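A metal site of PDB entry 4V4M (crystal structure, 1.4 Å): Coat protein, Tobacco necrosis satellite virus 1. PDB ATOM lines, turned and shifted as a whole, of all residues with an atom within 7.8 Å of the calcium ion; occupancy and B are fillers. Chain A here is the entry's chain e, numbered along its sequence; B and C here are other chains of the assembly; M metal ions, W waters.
The side-chain carboxylate (OE2) of Glu 26 of chain B lies within hydrogen-bond range of the side-chain amide nitrogen (NE2) of Gln 122 of chain C (2.9 Å).
The side-chain amino group (NZ) of Lys 28 of chain B lies within hydrogen-bond range of the side-chain hydroxyl (OG) of Ser 62.
The backbone NH of Glu 26 of chain B is in hydrogen-bond range of the chain-end carboxylate of Ala 196.
The side-chain carboxylate of Asp 195 of chain A is in salt-bridge range of the side-chain amino group of Lys 28 of chain A.
N of Asp 64 sits at hydrogen-bond distance from OE2 of Glu 26 of chain B (2.8 Å).
Within 4 Å of the calcium ion: Ser 62, Gln 65, Asp 195 of chain A and Glu 26 of chain B.
The nearest printed residue that does not touch the calcium ion is Ala 196 (4.4 Å).
The calcium ion is bound by OD2 of Asp 195 of chain A (2.3 Å), O of Ser 62 (2.3 Å), OE1 of Glu 26 of chain B (2.3 Å), O of Gln 65 (2.4 Å), water W2 (2.4 Å) and water W1 (2.4 Å).
The calcium ion has six donor atoms within binding distance.
Water W1 bridges the backbone carbonyl oxygen (O) of Asp 195 of chain A (2.9 Å) and the chain-end carboxylate (OXT) of Ala 196 (3.3 Å).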
ATOM      1  N   LYS A  28     -30.298  30.182  -0.430  1.00  0.00           N
ATOM      2  CA  LYS A  28     -29.103  30.961  -0.577  1.00  0.00           C
ATOM      3  C   LYS A  28     -28.339  30.476  -1.813  1.00  0.00           C
ATOM      4  O   LYS A  28     -28.641  29.412  -2.361  1.00  0.00           O
ATOM      5  CB  LYS A  28     -28.274  30.861   0.703  1.00  0.00           C
ATOM      6  CG  LYS A  28     -28.934  31.599   1.878  1.00  0.00           C
ATOM      7  CD  LYS A  28     -28.086  31.539   3.171  1.00  0.00           C
ATOM      8  CE  LYS A  28     -28.816  32.227   4.342  1.00  0.00           C
ATOM      9  NZ  LYS A  28     -28.057  32.167   5.606  1.00  0.00           N
ATOM     10  N   GLN A  60     -23.308  33.086   2.221  1.00  0.00           N
ATOM     11  CA  GLN A  60     -22.665  32.648   3.468  1.00  0.00           C
ATOM     12  C   GLN A  60     -23.569  31.677   4.229  1.00  0.00           C
ATOM     13  O   GLN A  60     -24.585  31.241   3.703  1.00  0.00           O
ATOM     14  CB  GLN A  60     -22.278  33.878   4.298  1.00  0.00           C
ATOM     15  CG  GLN A  60     -21.291  34.785   3.531  1.00  0.00           C
ATOM     16  CD  GLN A  60     -20.893  36.036   4.299  1.00  0.00           C
ATOM     17  OE1 GLN A  60     -21.699  36.619   5.026  1.00  0.00           O
ATOM     18  NE2 GLN A  60     -19.659  36.460   4.114  1.00  0.00           N
ATOM     19  N   ARG A  61     -23.197  31.321   5.453  1.00  0.00           N
ATOM     20  CA  ARG A  61     -23.962  30.334   6.209  1.00  0.00           C
ATOM     21  C   ARG A  61     -24.014  30.650   7.695  1.00  0.00           C
ATOM     22  O   ARG A  61     -23.088  31.256   8.258  1.00  0.00           O
ATOM     23  CB  ARG A  61     -23.388  28.926   6.022  1.00  0.00           C
ATOM     24  CG  ARG A  61     -21.915  28.825   6.433  1.00  0.00           C
ATOM     25  CD  ARG A  61     -21.341  27.417   6.246  1.00  0.00           C
ATOM     26  NE  ARG A  61     -19.878  27.450   6.200  1.00  0.00           N
ATOM     27  CZ  ARG A  61     -19.078  27.247   7.237  1.00  0.00           C
ATOM     28  NH1 ARG A  61     -19.577  26.944   8.451  1.00  0.00           N
ATOM     29  NH2 ARG A  61     -17.758  27.336   7.067  1.00  0.00           N
ATOM     30  N   SER A  62     -25.095  30.187   8.327  1.00  0.00           N
ATOM     31  CA  SER A  62     -25.215  30.178   9.771  1.00  0.00           C
ATOM     32  C   SER A  62     -24.832  28.785  10.234  1.00  0.00           C
ATOM     33  O   SER A  62     -25.304  27.808   9.659  1.00  0.00           O
ATOM     34  CB  SER A  62     -26.659  30.470  10.186  1.00  0.00           C
ATOM     35  OG  SER A  62     -26.816  30.487  11.593  1.00  0.00           O
ATOM     36  N   GLY A  63     -23.960  28.675  11.218  1.00  0.00           N
ATOM     37  CA  GLY A  63     -23.570  27.348  11.717  1.00  0.00           C
ATOM     38  C   GLY A  63     -22.622  26.574  10.805  1.00  0.00           C
ATOM     39  O   GLY A  63     -21.929  27.155   9.999  1.00  0.00           O
ATOM     40  N   ASP A  64     -22.602  25.258  10.975  1.00  0.00           N
ATOM     41  CA  ASP A  64     -21.633  24.397  10.302  1.00  0.00           C
ATOM     42  C   ASP A  64     -22.299  23.382   9.353  1.00  0.00           C
ATOM     43  O   ASP A  64     -21.682  22.407   8.959  1.00  0.00           O
ATOM     44  CB  ASP A  64     -20.726  23.678  11.312  1.00  0.00           C
ATOM     45  CG  ASP A  64     -19.591  24.553  11.830  1.00  0.00           C
ATOM     46  OD1 ASP A  64     -19.208  25.555  11.151  1.00  0.00           O
ATOM     47  OD2 ASP A  64     -19.057  24.229  12.918  1.00  0.00           O
ATOM     48  N   GLN A  65     -23.555  23.618   8.994  1.00  0.00           N
ATOM     49  CA  GLN A  65     -24.243  22.815   7.978  1.00  0.00           C
ATOM     50  C   GLN A  65     -25.000  23.679   6.993  1.00  0.00           C
ATOM     51  O   GLN A  65     -25.546  24.733   7.349  1.00  0.00           O
ATOM     52  CB  GLN A  65     -25.251  21.843   8.611  1.00  0.00           C
ATOM     53  CG  GLN A  65     -24.657  20.687   9.403  1.00  0.00           C
ATOM     54  CD  GLN A  65     -25.705  19.670   9.833  1.00  0.00           C
ATOM     55  OE1 GLN A  65     -26.886  19.994   9.932  1.00  0.00           O
ATOM     56  NE2 GLN A  65     -25.284  18.448  10.075  1.00  0.00           N
ATOM     57  N   VAL A  66     -25.027  23.210   5.751  1.00  0.00           N
ATOM     58  CA  VAL A  66     -25.973  23.691   4.759  1.00  0.00           C
ATOM     59  C   VAL A  66     -26.442  22.479   3.975  1.00  0.00           C
ATOM     60  O   VAL A  66     -25.872  21.398   4.097  1.00  0.00           O
ATOM     61  CB  VAL A  66     -25.368  24.733   3.779  1.00  0.00           C
ATOM     62  CG1 VAL A  66     -24.838  25.961   4.506  1.00  0.00           C
ATOM     63  CG2 VAL A  66     -24.312  24.075   2.925  1.00  0.00           C
ATOM     64  N   ARG A  67     -27.500  22.652   3.199  1.00  0.00           N
ATOM     65  CA  ARG A  67     -28.021  21.548   2.370  1.00  0.00           C
ATOM     66  C   ARG A  67     -28.081  22.031   0.929  1.00  0.00           C
ATOM     67  O   ARG A  67     -28.869  22.890   0.587  1.00  0.00           O
ATOM     68  CB  ARG A  67     -29.393  21.069   2.869  1.00  0.00           C
ATOM     69  CG  ARG A  67     -29.974  19.918   2.026  1.00  0.00           C
ATOM     70  CD  ARG A  67     -31.294  19.398   2.592  1.00  0.00           C
ATOM     71  NE  ARG A  67     -31.114  18.622   3.829  1.00  0.00           N
ATOM     72  CZ  ARG A  67     -30.641  17.374   3.847  1.00  0.00           C
ATOM     73  NH1 ARG A  67     -30.317  16.777   2.708  1.00  0.00           N
ATOM     74  NH2 ARG A  67     -30.491  16.730   4.996  1.00  0.00           N
ATOM     75  N   VAL A 155     -23.945  19.402   3.449  1.00  0.00           N
ATOM     76  CA  VAL A 155     -22.520  19.705   3.598  1.00  0.00           C
ATOM     77  C   VAL A 155     -22.287  20.115   5.055  1.00  0.00           C
ATOM     78  O   VAL A 155     -22.978  20.999   5.587  1.00  0.00           O
ATOM     79  CB  VAL A 155     -22.076  20.880   2.691  1.00  0.00           C
ATOM     80  CG1 VAL A 155     -20.583  21.174   2.897  1.00  0.00           C
ATOM     81  CG2 VAL A 155     -22.376  20.583   1.233  1.00  0.00           C
ATOM     82  N   TYR A 157     -19.352  21.420   7.934  1.00  0.00           N
ATOM     83  CA  TYR A 157     -18.098  22.185   8.007  1.00  0.00           C
ATOM     84  C   TYR A 157     -17.425  21.962   9.365  1.00  0.00           C
ATOM     85  O   TYR A 157     -18.088  21.610  10.352  1.00  0.00           O
ATOM     86  CB  TYR A 157     -18.337  23.688   7.784  1.00  0.00           C
ATOM     87  CG  TYR A 157     -18.752  24.019   6.377  1.00  0.00           C
ATOM     88  CD1 TYR A 157     -20.065  23.880   5.958  1.00  0.00           C
ATOM     89  CD2 TYR A 157     -17.802  24.489   5.452  1.00  0.00           C
ATOM     90  CE1 TYR A 157     -20.434  24.170   4.658  1.00  0.00           C
ATOM     91  CE2 TYR A 157     -18.167  24.802   4.161  1.00  0.00           C
ATOM     92  CZ  TYR A 157     -19.485  24.629   3.778  1.00  0.00           C
ATOM     93  OH  TYR A 157     -19.875  24.913   2.469  1.00  0.00           O
ATOM     94  N   TYR A 193     -28.441  26.530  -1.955  1.00  0.00           N
ATOM     95  CA  TYR A 193     -28.535  25.713  -0.746  1.00  0.00           C
ATOM     96  C   TYR A 193     -29.494  26.331   0.280  1.00  0.00           C
ATOM     97  O   TYR A 193     -29.696  27.531   0.290  1.00  0.00           O
ATOM     98  CB  TYR A 193     -27.136  25.553  -0.097  1.00  0.00           C
ATOM     99  CG  TYR A 193     -26.435  26.874   0.218  1.00  0.00           C
ATOM    100  CD1 TYR A 193     -25.739  27.583  -0.771  1.00  0.00           C
ATOM    101  CD2 TYR A 193     -26.455  27.415   1.507  1.00  0.00           C
ATOM    102  CE1 TYR A 193     -25.109  28.794  -0.488  1.00  0.00           C
ATOM    103  CE2 TYR A 193     -25.811  28.602   1.797  1.00  0.00           C
ATOM    104  CZ  TYR A 193     -25.134  29.289   0.797  1.00  0.00           C
ATOM    105  OH  TYR A 193     -24.524  30.486   1.078  1.00  0.00           O
ATOM    106  N   THR A 194     -30.117  25.490   1.100  1.00  0.00           N
ATOM    107  CA  THR A 194     -30.829  26.000   2.246  1.00  0.00           C
ATOM    108  C   THR A 194     -29.927  25.976   3.471  1.00  0.00           C
ATOM    109  O   THR A 194     -28.896  25.300   3.498  1.00  0.00           O
ATOM    110  CB  THR A 194     -32.122  25.210   2.532  1.00  0.00           C
ATOM    111  OG1 THR A 194     -31.778  23.849   2.824  1.00  0.00           O
ATOM    112  CG2 THR A 194     -33.074  25.298   1.332  1.00  0.00           C
ATOM    113  N   ASP A 195     -30.341  26.705   4.498  1.00  0.00           N
ATOM    114  CA  ASP A 195     -29.464  26.950   5.625  1.00  0.00           C
ATOM    115  C   ASP A 195     -30.334  27.191   6.850  1.00  0.00           C
ATOM    116  O   ASP A 195     -30.108  28.144   7.585  1.00  0.00           O
ATOM    117  CB  ASP A 195     -28.597  28.181   5.313  1.00  0.00           C
ATOM    118  CG  ASP A 195     -27.577  28.478   6.404  1.00  0.00           C
ATOM    119  OD1 ASP A 195     -27.274  29.684   6.628  1.00  0.00           O
ATOM    120  OD2 ASP A 195     -27.084  27.521   7.020  1.00  0.00           O
ATOM    121  N   ALA A 196     -31.315  26.311   7.060  1.00  0.00           N
ATOM    122  CA  ALA A 196     -32.280  26.447   8.155  1.00  0.00           C
ATOM    123  C   ALA A 196     -31.873  25.680   9.411  1.00  0.00           C
ATOM    124  O   ALA A 196     -32.584  25.776  10.427  1.00  0.00           O
ATOM    125  CB  ALA A 196     -33.638  25.985   7.686  1.00  0.00           C
ATOM    126  OXT ALA A 196     -30.894  24.953   9.452  1.00  0.00           O
ATOM    127  N   HIS B  24     -34.244  19.021   7.665  1.00  0.00           N
ATOM    128  CA  HIS B  24     -33.889  20.229   6.913  1.00  0.00           C
ATOM    129  C   HIS B  24     -33.306  21.289   7.836  1.00  0.00           C
ATOM    130  O   HIS B  24     -32.873  22.348   7.371  1.00  0.00           O
ATOM    131  CB  HIS B  24     -35.126  20.807   6.215  1.00  0.00           C
ATOM    132  CG  HIS B  24     -35.634  19.964   5.094  1.00  0.00           C
ATOM    133  ND1 HIS B  24     -35.489  20.315   3.770  1.00  0.00           N
ATOM    134  CD2 HIS B  24     -36.284  18.768   5.099  1.00  0.00           C
ATOM    135  CE1 HIS B  24     -36.035  19.388   3.007  1.00  0.00           C
ATOM    136  NE2 HIS B  24     -36.518  18.437   3.788  1.00  0.00           N
ATOM    137  N   LEU B  25     -33.309  21.009   9.125  1.00  0.00           N
ATOM    138  CA  LEU B  25     -32.867  21.976  10.117  1.00  0.00           C
ATOM    139  C   LEU B  25     -31.534  21.570  10.702  1.00  0.00           C
ATOM    140  O   LEU B  25     -31.381  20.433  11.162  1.00  0.00           O
ATOM    141  CB  LEU B  25     -33.876  22.044  11.266  1.00  0.00           C
ATOM    142  CG  LEU B  25     -35.329  22.320  10.913  1.00  0.00           C
ATOM    143  CD1 LEU B  25     -36.071  22.593  12.216  1.00  0.00           C
ATOM    144  CD2 LEU B  25     -35.449  23.492   9.978  1.00  0.00           C
ATOM    145  N   GLU B  26     -30.584  22.508  10.750  1.00  0.00           N
ATOM    146  CA  GLU B  26     -29.311  22.241  11.402  1.00  0.00           C
ATOM    147  C   GLU B  26     -29.508  22.010  12.901  1.00  0.00           C
ATOM    148  O   GLU B  26     -30.153  22.801  13.587  1.00  0.00           O
ATOM    149  CB  GLU B  26     -28.313  23.382  11.207  1.00  0.00           C
ATOM    150  CG  GLU B  26     -26.985  23.125  11.946  1.00  0.00           C
ATOM    151  CD  GLU B  26     -25.853  24.082  11.570  1.00  0.00           C
ATOM    152  OE1 GLU B  26     -25.982  24.825  10.560  1.00  0.00           O
ATOM    153  OE2 GLU B  26     -24.829  24.086  12.272  1.00  0.00           O
ATOM    154  N   HIS B  27     -28.953  20.908  13.404  1.00  0.00           N
ATOM    155  CA  HIS B  27     -28.944  20.684  14.846  1.00  0.00           C
ATOM    156  C   HIS B  27     -27.641  21.243  15.398  1.00  0.00           C
ATOM    157  O   HIS B  27     -26.608  20.585  15.374  1.00  0.00           O
ATOM    158  CB  HIS B  27     -29.147  19.198  15.151  1.00  0.00           C
ATOM    159  CG  HIS B  27     -30.534  18.738  14.790  1.00  0.00           C
ATOM    160  ND1 HIS B  27     -31.298  17.946  15.620  1.00  0.00           N
ATOM    161  CD2 HIS B  27     -31.297  18.990  13.708  1.00  0.00           C
ATOM    162  CE1 HIS B  27     -32.472  17.722  15.060  1.00  0.00           C
ATOM    163  NE2 HIS B  27     -32.488  18.336  13.890  1.00  0.00           N
ATOM    164  N   LYS B  28     -27.704  22.505  15.795  1.00  0.00           N
ATOM    165  CA  LYS B  28     -26.592  23.182  16.429  1.00  0.00           C
ATOM    166  C   LYS B  28     -26.333  22.552  17.790  1.00  0.00           C
ATOM    167  O   LYS B  28     -27.169  21.831  18.314  1.00  0.00           O
ATOM    168  CB  LYS B  28     -26.885  24.688  16.519  1.00  0.00           C
ATOM    169  CG  LYS B  28     -26.841  25.396  15.143  1.00  0.00           C
ATOM    170  CD  LYS B  28     -27.153  26.896  15.225  1.00  0.00           C
ATOM    171  CE  LYS B  28     -26.960  27.593  13.862  1.00  0.00           C
ATOM    172  NZ  LYS B  28     -27.325  29.040  13.926  1.00  0.00           N
ATOM    173  N   ASP B  56     -22.782  33.403  14.476  1.00  0.00           N
ATOM    174  CA  ASP B  56     -22.921  32.539  13.312  1.00  0.00           C
ATOM    175  C   ASP B  56     -22.323  31.138  13.525  1.00  0.00           C
ATOM    176  O   ASP B  56     -22.376  30.298  12.620  1.00  0.00           O
ATOM    177  CB  ASP B  56     -22.248  33.174  12.082  1.00  0.00           C
ATOM    178  CG  ASP B  56     -22.793  34.565  11.744  1.00  0.00           C
ATOM    179  OD1 ASP B  56     -23.972  34.848  12.026  1.00  0.00           O
ATOM    180  OD2 ASP B  56     -22.018  35.349  11.158  1.00  0.00           O
ATOM    181  N   ASP B 195     -32.483  26.107  15.150  1.00  0.00           N
ATOM    182  CA  ASP B 195     -32.400  27.556  15.207  1.00  0.00           C
ATOM    183  C   ASP B 195     -32.920  28.114  13.899  1.00  0.00           C
ATOM    184  O   ASP B 195     -32.290  28.977  13.268  1.00  0.00           O
ATOM    185  CB  ASP B 195     -30.936  27.944  15.442  1.00  0.00           C
ATOM    186  CG  ASP B 195     -30.736  29.433  15.598  1.00  0.00           C
ATOM    187  OD1 ASP B 195     -29.658  29.911  15.202  1.00  0.00           O
ATOM    188  OD2 ASP B 195     -31.622  30.126  16.124  1.00  0.00           O
ATOM    189  N   GLN C 122     -21.974  16.564  15.640  1.00  0.00           N
ATOM    190  CA  GLN C 122     -22.982  17.069  14.703  1.00  0.00           C
ATOM    191  C   GLN C 122     -22.887  16.371  13.347  1.00  0.00           C
ATOM    192  O   GLN C 122     -23.896  15.977  12.777  1.00  0.00           O
ATOM    193  CB  GLN C 122     -22.827  18.579  14.455  1.00  0.00           C
ATOM    194  CG  GLN C 122     -23.821  19.123  13.404  1.00  0.00           C
ATOM    195  CD  GLN C 122     -23.557  20.566  13.012  1.00  0.00           C
ATOM    196  OE1 GLN C 122     -22.562  20.885  12.327  1.00  0.00           O
ATOM    197  NE2 GLN C 122     -24.466  21.456  13.403  1.00  0.00           N
HETATM  198 CA    CA M   1     -26.724  26.165   8.793  1.00  0.00          CA
HETATM  199  O   HOH W   1     -28.572  27.306   9.905  1.00  0.00           O
HETATM  200  O   HOH W   2     -28.529  24.767   8.165  1.00  0.00           O
